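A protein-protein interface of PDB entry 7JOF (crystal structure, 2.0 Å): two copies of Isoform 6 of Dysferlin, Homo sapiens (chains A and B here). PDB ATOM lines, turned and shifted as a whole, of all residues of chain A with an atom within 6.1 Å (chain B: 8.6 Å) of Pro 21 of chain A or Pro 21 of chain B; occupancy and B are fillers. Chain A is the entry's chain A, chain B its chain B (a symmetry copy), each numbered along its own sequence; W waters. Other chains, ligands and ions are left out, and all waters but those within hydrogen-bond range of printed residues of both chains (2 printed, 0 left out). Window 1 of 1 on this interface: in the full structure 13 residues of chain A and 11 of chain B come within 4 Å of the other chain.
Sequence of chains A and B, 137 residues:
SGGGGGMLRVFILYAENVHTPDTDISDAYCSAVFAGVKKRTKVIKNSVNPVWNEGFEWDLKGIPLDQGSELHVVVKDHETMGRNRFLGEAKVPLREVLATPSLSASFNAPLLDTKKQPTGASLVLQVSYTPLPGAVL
OD2 of Asp 113 of chain B lies within hydrogen-bond range of OG1 of Thr 23 of chain A, at 2.9 Å.
OG1 of Thr 114 of chain B lies within hydrogen-bond range of NH2 of Arg 85 of chain A.
OD2 of Asp 22 of chain A sits at hydrogen-bond distance from OG1 of Thr 114 of chain B (2.7 Å).
The side-chain carboxylate (OD2) of Asp 24 of chain A lies close to the guanidinium group (NH2) of Arg 85 of chain A (3.4 Å).
The side-chain carboxylate of Asp 22 of chain A sits at hydrogen-bond distance from the backbone NH of Asp 24 of chain A (3.1 Å).
The backbone NH (N) of Asp 22 of chain A sits at hydrogen-bond distance from the side-chain hydroxyl (OG1) of Thr 20 of chain A.
The side-chain carboxylate of Asp 22 of chain A is in salt-bridge range of the guanidinium group of Arg 85 of chain A (2.9 Å).
The backbone NH of Asp 77 of chain A lies within hydrogen-bond range of the backbone carbonyl oxygen of Arg 85 of chain A (2.7 Å).
N of Gln 117 of chain B is in hydrogen-bond range of OD1 of Asp 113 of chain B.
CG of Pro 21 of chain A touches CB of Pro 21 of chain B, 3.2 Å away.
OD2 of Asp 113 of chain B touches CB of Asp 22 of chain A, at 3.2 Å.
OG1 of Thr 23 of chain A touches CG of Gln 117 of chain B (3.6 Å).
Of chain B, only Pro 21 comes within 4 Å of Pro 21 of chain A.
No residue of chain B comes within 4 Å of Thr 20 of chain A.
Asp 22 of chain A touches just these residues of chain B: Asp 113 and Thr 114.
Of the printed residues of chain A, Asp 113 of chain B touches Asp 22 and Thr 23.
Printed residues of chain A within 4 Å of Gln 117 of chain B: Thr 23 (3.6 Å).
The nearest residue of chain B that does not touch Pro 21 of chain A is Asp 113 of chain B (5.8 Å).
The nearest printed residue of chain A that does not touch Pro 21 of chain B is Phe 86 of chain A (5.5 Å).
Of the 21 printed residues of chain B, 4 touch a printed residue of chain A.
Of the 10 printed residues of chain A, 4 touch a printed residue of chain B.
Printed residues of chain A that touch a printed residue of chain B: Pro 21, Asp 22, Thr 23 and Arg 85.
Hydrophobic or aromatic side chains of chain A that line the printed part of chain B: Pro 21.
Among the printed residues, no Asp or Glu carboxylate lies within 4 Å of a Lys or Arg side-chain nitrogen of the other chain.
Pro 21 of chain A touches its own counterpart, Pro 21 of chain B.
Positions printed for both chains: 19, 20, 21, 22, 23, 24, 77, 85, 86 and 87.
Of the 6 pairs that touch across the chains among the printed residues, 1 has its exchanged pair printed and touching as well.
Water W1 bridges the backbone NH (N) of Phe 86 of chain A (2.9 Å) and the guanidinium group (NH2) of Arg 83 of chain B (3.0 Å).
Water W2 lies within hydrogen-bond range of the side-chain hydroxyl (OG1) of Thr 114 of chain B and the guanidinium group (NH2) of Arg 85 of chain A.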
ATOM      1  N   HIS A  19       9.366  10.628  24.032  1.00  0.00           N
ATOM      2  CA  HIS A  19       9.770   9.344  23.403  1.00  0.00           C
ATOM      3  C   HIS A  19       8.555   8.524  22.962  1.00  0.00           C
ATOM      4  O   HIS A  19       7.651   8.299  23.776  1.00  0.00           O
ATOM      5  CB  HIS A  19      10.668   8.538  24.350  1.00  0.00           C
ATOM      6  CG  HIS A  19      11.998   9.165  24.606  1.00  0.00           C
ATOM      7  ND1 HIS A  19      12.274   9.855  25.757  1.00  0.00           N
ATOM      8  CD2 HIS A  19      13.117   9.219  23.858  1.00  0.00           C
ATOM      9  CE1 HIS A  19      13.510  10.296  25.722  1.00  0.00           C
ATOM     10  NE2 HIS A  19      14.045   9.928  24.568  1.00  0.00           N
ATOM     11  N   THR A  20       8.615   8.032  21.737  1.00  0.00           N
ATOM     12  CA  THR A  20       7.536   7.175  21.194  1.00  0.00           C
ATOM     13  C   THR A  20       7.668   5.763  21.730  1.00  0.00           C
ATOM     14  O   THR A  20       8.707   5.401  22.280  1.00  0.00           O
ATOM     15  CB  THR A  20       7.581   7.022  19.668  1.00  0.00           C
ATOM     16  OG1 THR A  20       8.606   6.141  19.239  1.00  0.00           O
ATOM     17  CG2 THR A  20       7.726   8.336  18.959  1.00  0.00           C
ATOM     18  N   PRO A  21       6.682   4.959  21.383  1.00  0.00           N
ATOM     19  CA  PRO A  21       6.713   3.553  21.808  1.00  0.00           C
ATOM     20  C   PRO A  21       7.633   2.622  21.002  1.00  0.00           C
ATOM     21  O   PRO A  21       7.524   1.425  21.195  1.00  0.00           O
ATOM     22  CB  PRO A  21       5.255   3.110  21.631  1.00  0.00           C
ATOM     23  CG  PRO A  21       4.469   4.340  22.007  1.00  0.00           C
ATOM     24  CD  PRO A  21       5.323   5.498  21.529  1.00  0.00           C
ATOM     25  N   ASP A  22       8.523   3.106  20.130  1.00  0.00           N
ATOM     26  CA  ASP A  22       9.411   2.193  19.357  1.00  0.00           C
ATOM     27  C   ASP A  22      10.625   2.955  18.815  1.00  0.00           C
ATOM     28  O   ASP A  22      10.965   3.947  19.381  1.00  0.00           O
ATOM     29  CB  ASP A  22       8.687   1.447  18.235  1.00  0.00           C
ATOM     30  CG  ASP A  22       7.826   2.347  17.385  1.00  0.00           C
ATOM     31  OD1 ASP A  22       8.176   3.488  17.249  1.00  0.00           O
ATOM     32  OD2 ASP A  22       6.832   1.885  16.916  1.00  0.00           O
ATOM     33  N   THR A  23      11.175   2.503  17.686  1.00  0.00           N
ATOM     34  CA  THR A  23      12.393   3.087  17.059  1.00  0.00           C
ATOM     35  C   THR A  23      12.117   4.442  16.373  1.00  0.00           C
ATOM     36  O   THR A  23      13.058   5.146  16.101  1.00  0.00           O
ATOM     37  CB  THR A  23      13.060   2.072  16.123  1.00  0.00           C
ATOM     38  OG1 THR A  23      12.129   1.855  15.069  1.00  0.00           O
ATOM     39  CG2 THR A  23      13.476   0.793  16.823  1.00  0.00           C
ATOM     40  N   ASP A  24      10.837   4.748  16.132  1.00  0.00           N
ATOM     41  CA  ASP A  24      10.433   6.022  15.479  1.00  0.00           C
ATOM     42  C   ASP A  24      10.791   7.198  16.394  1.00  0.00           C
ATOM     43  O   ASP A  24      10.597   7.075  17.620  1.00  0.00           O
ATOM     44  CB  ASP A  24       8.945   6.015  15.117  1.00  0.00           C
ATOM     45  CG  ASP A  24       8.443   7.353  14.604  1.00  0.00           C
ATOM     46  OD1 ASP A  24       9.045   7.877  13.646  1.00  0.00           O
ATOM     47  OD2 ASP A  24       7.452   7.862  15.167  1.00  0.00           O
ATOM     48  N   ASP A  77       1.871  11.430  19.068  1.00  0.00           N
ATOM     49  CA  ASP A  77       2.880  11.174  18.021  1.00  0.00           C
ATOM     50  C   ASP A  77       2.169  10.994  16.679  1.00  0.00           C
ATOM     51  O   ASP A  77       1.430  10.029  16.527  1.00  0.00           O
ATOM     52  CB  ASP A  77       3.796  10.006  18.340  1.00  0.00           C
ATOM     53  CG  ASP A  77       4.527   9.565  17.084  1.00  0.00           C
ATOM     54  OD1 ASP A  77       5.244  10.391  16.507  1.00  0.00           O
ATOM     55  OD2 ASP A  77       4.321   8.428  16.694  1.00  0.00           O
ATOM     56  N   ARG A  85      -0.674   8.343  17.856  1.00  0.00           N
ATOM     57  CA  ARG A  85      -0.555   7.573  19.119  1.00  0.00           C
ATOM     58  C   ARG A  85      -0.273   8.496  20.317  1.00  0.00           C
ATOM     59  O   ARG A  85       0.511   9.418  20.212  1.00  0.00           O
ATOM     60  CB  ARG A  85       0.460   6.440  18.970  1.00  0.00           C
ATOM     61  CG  ARG A  85       1.613   6.767  18.036  1.00  0.00           C
ATOM     62  CD  ARG A  85       2.412   5.587  17.534  1.00  0.00           C
ATOM     63  NE  ARG A  85       3.823   5.825  17.589  1.00  0.00           N
ATOM     64  CZ  ARG A  85       4.751   4.934  17.284  1.00  0.00           C
ATOM     65  NH1 ARG A  85       4.701   3.693  17.745  1.00  0.00           N
ATOM     66  NH2 ARG A  85       5.742   5.314  16.524  1.00  0.00           N
ATOM     67  N   PHE A  86      -0.944   8.204  21.421  1.00  0.00           N
ATOM     68  CA  PHE A  86      -0.838   8.980  22.672  1.00  0.00           C
ATOM     69  C   PHE A  86       0.582   8.824  23.238  1.00  0.00           C
ATOM     70  O   PHE A  86       1.097   7.759  23.290  1.00  0.00           O
ATOM     71  CB  PHE A  86      -1.908   8.492  23.635  1.00  0.00           C
ATOM     72  CG  PHE A  86      -1.819   9.071  25.012  1.00  0.00           C
ATOM     73  CD1 PHE A  86      -1.027   8.502  25.975  1.00  0.00           C
ATOM     74  CD2 PHE A  86      -2.484  10.231  25.313  1.00  0.00           C
ATOM     75  CE1 PHE A  86      -0.978   9.063  27.223  1.00  0.00           C
ATOM     76  CE2 PHE A  86      -2.411  10.783  26.570  1.00  0.00           C
ATOM     77  CZ  PHE A  86      -1.651  10.206  27.524  1.00  0.00           C
ATOM     78  N   LEU A  87       1.189   9.921  23.631  1.00  0.00           N
ATOM     79  CA  LEU A  87       2.552   9.921  24.202  1.00  0.00           C
ATOM     80  C   LEU A  87       2.462  10.276  25.687  1.00  0.00           C
ATOM     81  O   LEU A  87       3.070   9.681  26.443  1.00  0.00           O
ATOM     82  CB  LEU A  87       3.443  10.896  23.434  1.00  0.00           C
ATOM     83  CG  LEU A  87       3.892  10.494  22.035  1.00  0.00           C
ATOM     84  CD1 LEU A  87       5.021  11.379  21.548  1.00  0.00           C
ATOM     85  CD2 LEU A  87       4.237   9.030  21.945  1.00  0.00           C
ATOM     86  N   VAL B  18       5.914  -9.037  25.237  1.00  0.00           N
ATOM     87  CA  VAL B  18       5.032  -8.036  24.568  1.00  0.00           C
ATOM     88  C   VAL B  18       4.744  -6.976  25.625  1.00  0.00           C
ATOM     89  O   VAL B  18       4.115  -7.306  26.643  1.00  0.00           O
ATOM     90  CB  VAL B  18       3.727  -8.648  24.017  1.00  0.00           C
ATOM     91  CG1 VAL B  18       3.990  -9.739  22.996  1.00  0.00           C
ATOM     92  CG2 VAL B  18       2.835  -9.170  25.117  1.00  0.00           C
ATOM     93  N   HIS B  19       5.194  -5.751  25.374  1.00  0.00           N
ATOM     94  CA  HIS B  19       5.020  -4.659  26.360  1.00  0.00           C
ATOM     95  C   HIS B  19       4.303  -3.454  25.748  1.00  0.00           C
ATOM     96  O   HIS B  19       4.478  -3.167  24.561  1.00  0.00           O
ATOM     97  CB  HIS B  19       6.387  -4.149  26.839  1.00  0.00           C
ATOM     98  CG  HIS B  19       7.221  -5.167  27.536  1.00  0.00           C
ATOM     99  ND1 HIS B  19       7.323  -5.213  28.900  1.00  0.00           N
ATOM    100  CD2 HIS B  19       7.994  -6.165  27.061  1.00  0.00           C
ATOM    101  CE1 HIS B  19       8.113  -6.203  29.244  1.00  0.00           C
ATOM    102  NE2 HIS B  19       8.543  -6.800  28.135  1.00  0.00           N
ATOM    103  N   THR B  20       3.529  -2.770  26.584  1.00  0.00           N
ATOM    104  CA  THR B  20       2.909  -1.474  26.205  1.00  0.00           C
ATOM    105  C   THR B  20       3.983  -0.367  26.295  1.00  0.00           C
ATOM    106  O   THR B  20       5.116  -0.642  26.720  1.00  0.00           O
ATOM    107  CB  THR B  20       1.710  -1.168  27.110  1.00  0.00           C
ATOM    108  OG1 THR B  20       2.226  -0.645  28.332  1.00  0.00           O
ATOM    109  CG2 THR B  20       0.846  -2.381  27.380  1.00  0.00           C
ATOM    110  N   PRO B  21       3.642   0.858  25.894  1.00  0.00           N
ATOM    111  CA  PRO B  21       4.614   1.955  25.976  1.00  0.00           C
ATOM    112  C   PRO B  21       4.616   2.616  27.365  1.00  0.00           C
ATOM    113  O   PRO B  21       5.416   3.500  27.593  1.00  0.00           O
ATOM    114  CB  PRO B  21       4.165   2.978  24.926  1.00  0.00           C
ATOM    115  CG  PRO B  21       2.700   2.712  24.753  1.00  0.00           C
ATOM    116  CD  PRO B  21       2.556   1.224  24.984  1.00  0.00           C
ATOM    117  N   ASP B  22       3.770   2.155  28.280  1.00  0.00           N
ATOM    118  CA  ASP B  22       3.695   2.866  29.584  1.00  0.00           C
ATOM    119  C   ASP B  22       3.585   1.875  30.747  1.00  0.00           C
ATOM    120  O   ASP B  22       3.824   0.679  30.552  1.00  0.00           O
ATOM    121  CB  ASP B  22       2.576   3.910  29.569  1.00  0.00           C
ATOM    122  CG  ASP B  22       1.204   3.311  29.310  1.00  0.00           C
ATOM    123  OD1 ASP B  22       1.071   2.090  29.455  1.00  0.00           O
ATOM    124  OD2 ASP B  22       0.296   4.068  28.949  1.00  0.00           O
ATOM    125  N   THR B  23       3.121   2.372  31.898  1.00  0.00           N
ATOM    126  CA  THR B  23       2.987   1.547  33.129  1.00  0.00           C
ATOM    127  C   THR B  23       1.897   0.479  32.951  1.00  0.00           C
ATOM    128  O   THR B  23       1.813  -0.388  33.800  1.00  0.00           O
ATOM    129  CB  THR B  23       2.855   2.404  34.396  1.00  0.00           C
ATOM    130  OG1 THR B  23       1.646   3.158  34.365  1.00  0.00           O
ATOM    131  CG2 THR B  23       4.043   3.318  34.610  1.00  0.00           C
ATOM    132  N   ASP B  24       1.083   0.579  31.901  1.00  0.00           N
ATOM    133  CA  ASP B  24       0.025  -0.438  31.667  1.00  0.00           C
ATOM    134  C   ASP B  24       0.681  -1.802  31.411  1.00  0.00           C
ATOM    135  O   ASP B  24       1.689  -1.841  30.697  1.00  0.00           O
ATOM    136  CB  ASP B  24      -0.878  -0.056  30.488  1.00  0.00           C
ATOM    137  CG  ASP B  24      -1.973  -1.067  30.158  1.00  0.00           C
ATOM    138  OD1 ASP B  24      -2.570  -1.606  31.085  1.00  0.00           O
ATOM    139  OD2 ASP B  24      -2.232  -1.271  28.972  1.00  0.00           O
ATOM    140  N   ILE B  25       0.139  -2.857  32.028  1.00  0.00           N
ATOM    141  CA  ILE B  25       0.603  -4.245  31.748  1.00  0.00           C
ATOM    142  C   ILE B  25      -0.247  -4.686  30.554  1.00  0.00           C
ATOM    143  O   ILE B  25      -1.464  -4.600  30.656  1.00  0.00           O
ATOM    144  CB  ILE B  25       0.429  -5.184  32.955  1.00  0.00           C
ATOM    145  CG1 ILE B  25       1.071  -4.629  34.225  1.00  0.00           C
ATOM    146  CG2 ILE B  25       0.961  -6.568  32.626  1.00  0.00           C
ATOM    147  CD1 ILE B  25       0.974  -5.573  35.392  1.00  0.00           C
ATOM    148  N   SER B  26       0.384  -5.231  29.522  1.00  0.00           N
ATOM    149  CA  SER B  26      -0.321  -5.508  28.247  1.00  0.00           C
ATOM    150  C   SER B  26      -1.596  -6.339  28.448  1.00  0.00           C
ATOM    151  O   SER B  26      -1.598  -7.293  29.222  1.00  0.00           O
ATOM    152  CB  SER B  26       0.623  -6.162  27.267  1.00  0.00           C
ATOM    153  OG  SER B  26       1.875  -5.496  27.239  1.00  0.00           O
ATOM    154  N   ASP B  77      -2.683  -4.038  22.260  1.00  0.00           N
ATOM    155  CA  ASP B  77      -3.042  -3.929  23.690  1.00  0.00           C
ATOM    156  C   ASP B  77      -4.454  -3.348  23.777  1.00  0.00           C
ATOM    157  O   ASP B  77      -4.676  -2.232  23.268  1.00  0.00           O
ATOM    158  CB  ASP B  77      -2.024  -3.062  24.426  1.00  0.00           C
ATOM    159  CG  ASP B  77      -2.573  -2.537  25.736  1.00  0.00           C
ATOM    160  OD1 ASP B  77      -2.956  -3.367  26.562  1.00  0.00           O
ATOM    161  OD2 ASP B  77      -2.635  -1.308  25.888  1.00  0.00           O
ATOM    162  N   GLU B  79      -7.575  -1.370  25.114  1.00  0.00           N
ATOM    163  CA  GLU B  79      -7.697  -0.152  25.962  1.00  0.00           C
ATOM    164  C   GLU B  79      -9.175   0.092  26.287  1.00  0.00           C
ATOM    165  O   GLU B  79     -10.019  -0.127  25.396  1.00  0.00           O
ATOM    166  CB  GLU B  79      -7.084   1.057  25.250  1.00  0.00           C
ATOM    167  CG  GLU B  79      -5.571   1.117  25.355  1.00  0.00           C
ATOM    168  CD  GLU B  79      -5.048   1.535  26.718  1.00  0.00           C
ATOM    169  OE1 GLU B  79      -4.863   2.748  26.932  1.00  0.00           O
ATOM    170  OE2 GLU B  79      -4.825   0.643  27.563  1.00  0.00           O
ATOM    171  N   ARG B  83      -8.069   4.323  22.240  1.00  0.00           N
ATOM    172  CA  ARG B  83      -7.942   3.402  21.093  1.00  0.00           C
ATOM    173  C   ARG B  83      -6.983   2.261  21.442  1.00  0.00           C
ATOM    174  O   ARG B  83      -6.026   2.527  22.130  1.00  0.00           O
ATOM    175  CB  ARG B  83      -7.548   4.176  19.841  1.00  0.00           C
ATOM    176  CG  ARG B  83      -6.543   3.515  18.915  1.00  0.00           C
ATOM    177  CD  ARG B  83      -5.703   4.594  18.280  1.00  0.00           C
ATOM    178  NE  ARG B  83      -4.342   4.657  18.755  1.00  0.00           N
ATOM    179  CZ  ARG B  83      -3.437   3.713  18.572  1.00  0.00           C
ATOM    180  NH1 ARG B  83      -3.481   2.914  17.520  1.00  0.00           N
ATOM    181  NH2 ARG B  83      -2.491   3.548  19.456  1.00  0.00           N
ATOM    182  N   ARG B  85      -3.830  -0.215  21.333  1.00  0.00           N
ATOM    183  CA  ARG B  85      -2.460   0.176  20.903  1.00  0.00           C
ATOM    184  C   ARG B  85      -1.717  -0.976  20.225  1.00  0.00           C
ATOM    185  O   ARG B  85      -1.688  -2.079  20.784  1.00  0.00           O
ATOM    186  CB  ARG B  85      -1.646   0.702  22.089  1.00  0.00           C
ATOM    187  CG  ARG B  85      -2.461   1.558  23.043  1.00  0.00           C
ATOM    188  CD  ARG B  85      -1.658   2.203  24.148  1.00  0.00           C
ATOM    189  NE  ARG B  85      -1.675   1.412  25.361  1.00  0.00           N
ATOM    190  CZ  ARG B  85      -1.108   1.785  26.498  1.00  0.00           C
ATOM    191  NH1 ARG B  85      -0.532   2.971  26.589  1.00  0.00           N
ATOM    192  NH2 ARG B  85      -1.118   0.978  27.541  1.00  0.00           N
ATOM    193  N   PHE B  86      -1.141  -0.684  19.059  1.00  0.00           N
ATOM    194  CA  PHE B  86      -0.328  -1.656  18.292  1.00  0.00           C
ATOM    195  C   PHE B  86       0.938  -1.942  19.111  1.00  0.00           C
ATOM    196  O   PHE B  86       1.561  -0.983  19.582  1.00  0.00           O
ATOM    197  CB  PHE B  86      -0.035  -1.060  16.910  1.00  0.00           C
ATOM    198  CG  PHE B  86       1.138  -1.646  16.171  1.00  0.00           C
ATOM    199  CD1 PHE B  86       2.436  -1.304  16.511  1.00  0.00           C
ATOM    200  CD2 PHE B  86       0.944  -2.528  15.120  1.00  0.00           C
ATOM    201  CE1 PHE B  86       3.513  -1.837  15.823  1.00  0.00           C
ATOM    202  CE2 PHE B  86       2.024  -3.070  14.443  1.00  0.00           C
ATOM    203  CZ  PHE B  86       3.306  -2.723  14.795  1.00  0.00           C
ATOM    204  N   LEU B  87       1.255  -3.221  19.320  1.00  0.00           N
ATOM    205  CA  LEU B  87       2.468  -3.621  20.080  1.00  0.00           C
ATOM    206  C   LEU B  87       3.523  -4.185  19.123  1.00  0.00           C
ATOM    207  O   LEU B  87       4.698  -3.851  19.269  1.00  0.00           O
ATOM    208  CB  LEU B  87       2.079  -4.685  21.103  1.00  0.00           C
ATOM    209  CG  LEU B  87       1.192  -4.220  22.251  1.00  0.00           C
ATOM    210  CD1 LEU B  87       1.076  -5.319  23.292  1.00  0.00           C
ATOM    211  CD2 LEU B  87       1.736  -2.944  22.866  1.00  0.00           C
ATOM    212  N   GLY B  88       3.096  -5.045  18.196  1.00  0.00           N
ATOM    213  CA  GLY B  88       4.028  -5.658  17.232  1.00  0.00           C
ATOM    214  C   GLY B  88       3.298  -6.432  16.150  1.00  0.00           C
ATOM    215  O   GLY B  88       2.189  -6.935  16.421  1.00  0.00           O
ATOM    216  N   ASP B 113       8.087  -3.398  14.830  1.00  0.00           N
ATOM    217  CA  ASP B 113       7.446  -2.130  15.252  1.00  0.00           C
ATOM    218  C   ASP B 113       6.828  -1.409  14.039  1.00  0.00           C
ATOM    219  O   ASP B 113       6.893  -1.918  12.959  1.00  0.00           O
ATOM    220  CB  ASP B 113       8.378  -1.276  16.116  1.00  0.00           C
ATOM    221  CG  ASP B 113       9.622  -0.705  15.450  1.00  0.00           C
ATOM    222  OD1 ASP B 113       9.748  -0.767  14.249  1.00  0.00           O
ATOM    223  OD2 ASP B 113      10.419  -0.176  16.162  1.00  0.00           O
ATOM    224  N   THR B 114       6.399  -0.167  14.227  1.00  0.00           N
ATOM    225  CA  THR B 114       5.785   0.664  13.158  1.00  0.00           C
ATOM    226  C   THR B 114       6.828   1.018  12.092  1.00  0.00           C
ATOM    227  O   THR B 114       6.426   1.426  10.999  1.00  0.00           O
ATOM    228  CB  THR B 114       5.143   1.930  13.741  1.00  0.00           C
ATOM    229  OG1 THR B 114       6.152   2.646  14.446  1.00  0.00           O
ATOM    230  CG2 THR B 114       3.982   1.632  14.665  1.00  0.00           C
ATOM    231  N   GLN B 117      11.255  -2.494  12.732  1.00  0.00           N
ATOM    232  CA  GLN B 117      12.439  -2.861  13.558  1.00  0.00           C
ATOM    233  C   GLN B 117      11.993  -3.826  14.665  1.00  0.00           C
ATOM    234  O   GLN B 117      10.879  -3.635  15.192  1.00  0.00           O
ATOM    235  CB  GLN B 117      13.086  -1.606  14.149  1.00  0.00           C
ATOM    236  CG  GLN B 117      13.689  -0.681  13.102  1.00  0.00           C
ATOM    237  CD  GLN B 117      14.795  -1.346  12.321  1.00  0.00           C
ATOM    238  OE1 GLN B 117      15.933  -1.441  12.776  1.00  0.00           O
ATOM    239  NE2 GLN B 117      14.465  -1.815  11.129  1.00  0.00           N
ATOM    240  N   PRO B 118      12.826  -4.820  15.002  1.00  0.00           N
ATOM    241  CA  PRO B 118      12.460  -5.779  16.043  1.00  0.00           C
ATOM    242  C   PRO B 118      12.147  -5.116  17.403  1.00  0.00           C
ATOM    243  O   PRO B 118      12.871  -4.309  17.869  1.00  0.00           O
ATOM    244  CB  PRO B 118      13.657  -6.721  16.176  1.00  0.00           C
ATOM    245  CG  PRO B 118      14.429  -6.491  14.899  1.00  0.00           C
ATOM    246  CD  PRO B 118      14.151  -5.066  14.504  1.00  0.00           C
ATOM    247  N   THR B 119      11.027  -5.533  17.986  1.00  0.00           N
ATOM    248  CA  THR B 119      10.524  -5.023  19.287  1.00  0.00           C
ATOM    249  C   THR B 119      11.126  -5.876  20.417  1.00  0.00           C
ATOM    250  O   THR B 119      11.060  -5.486  21.535  1.00  0.00           O
ATOM    251  CB  THR B 119       8.988  -5.029  19.310  1.00  0.00           C
ATOM    252  OG1 THR B 119       8.654  -6.356  19.667  1.00  0.00           O
ATOM    253  CG2 THR B 119       8.344  -4.677  17.984  1.00  0.00           C
HETATM  254  O   HOH W   1      -2.348   5.629  21.612  1.00  0.00           O
HETATM  255  O   HOH W   2       6.372   5.439  13.169  1.00  0.00           O
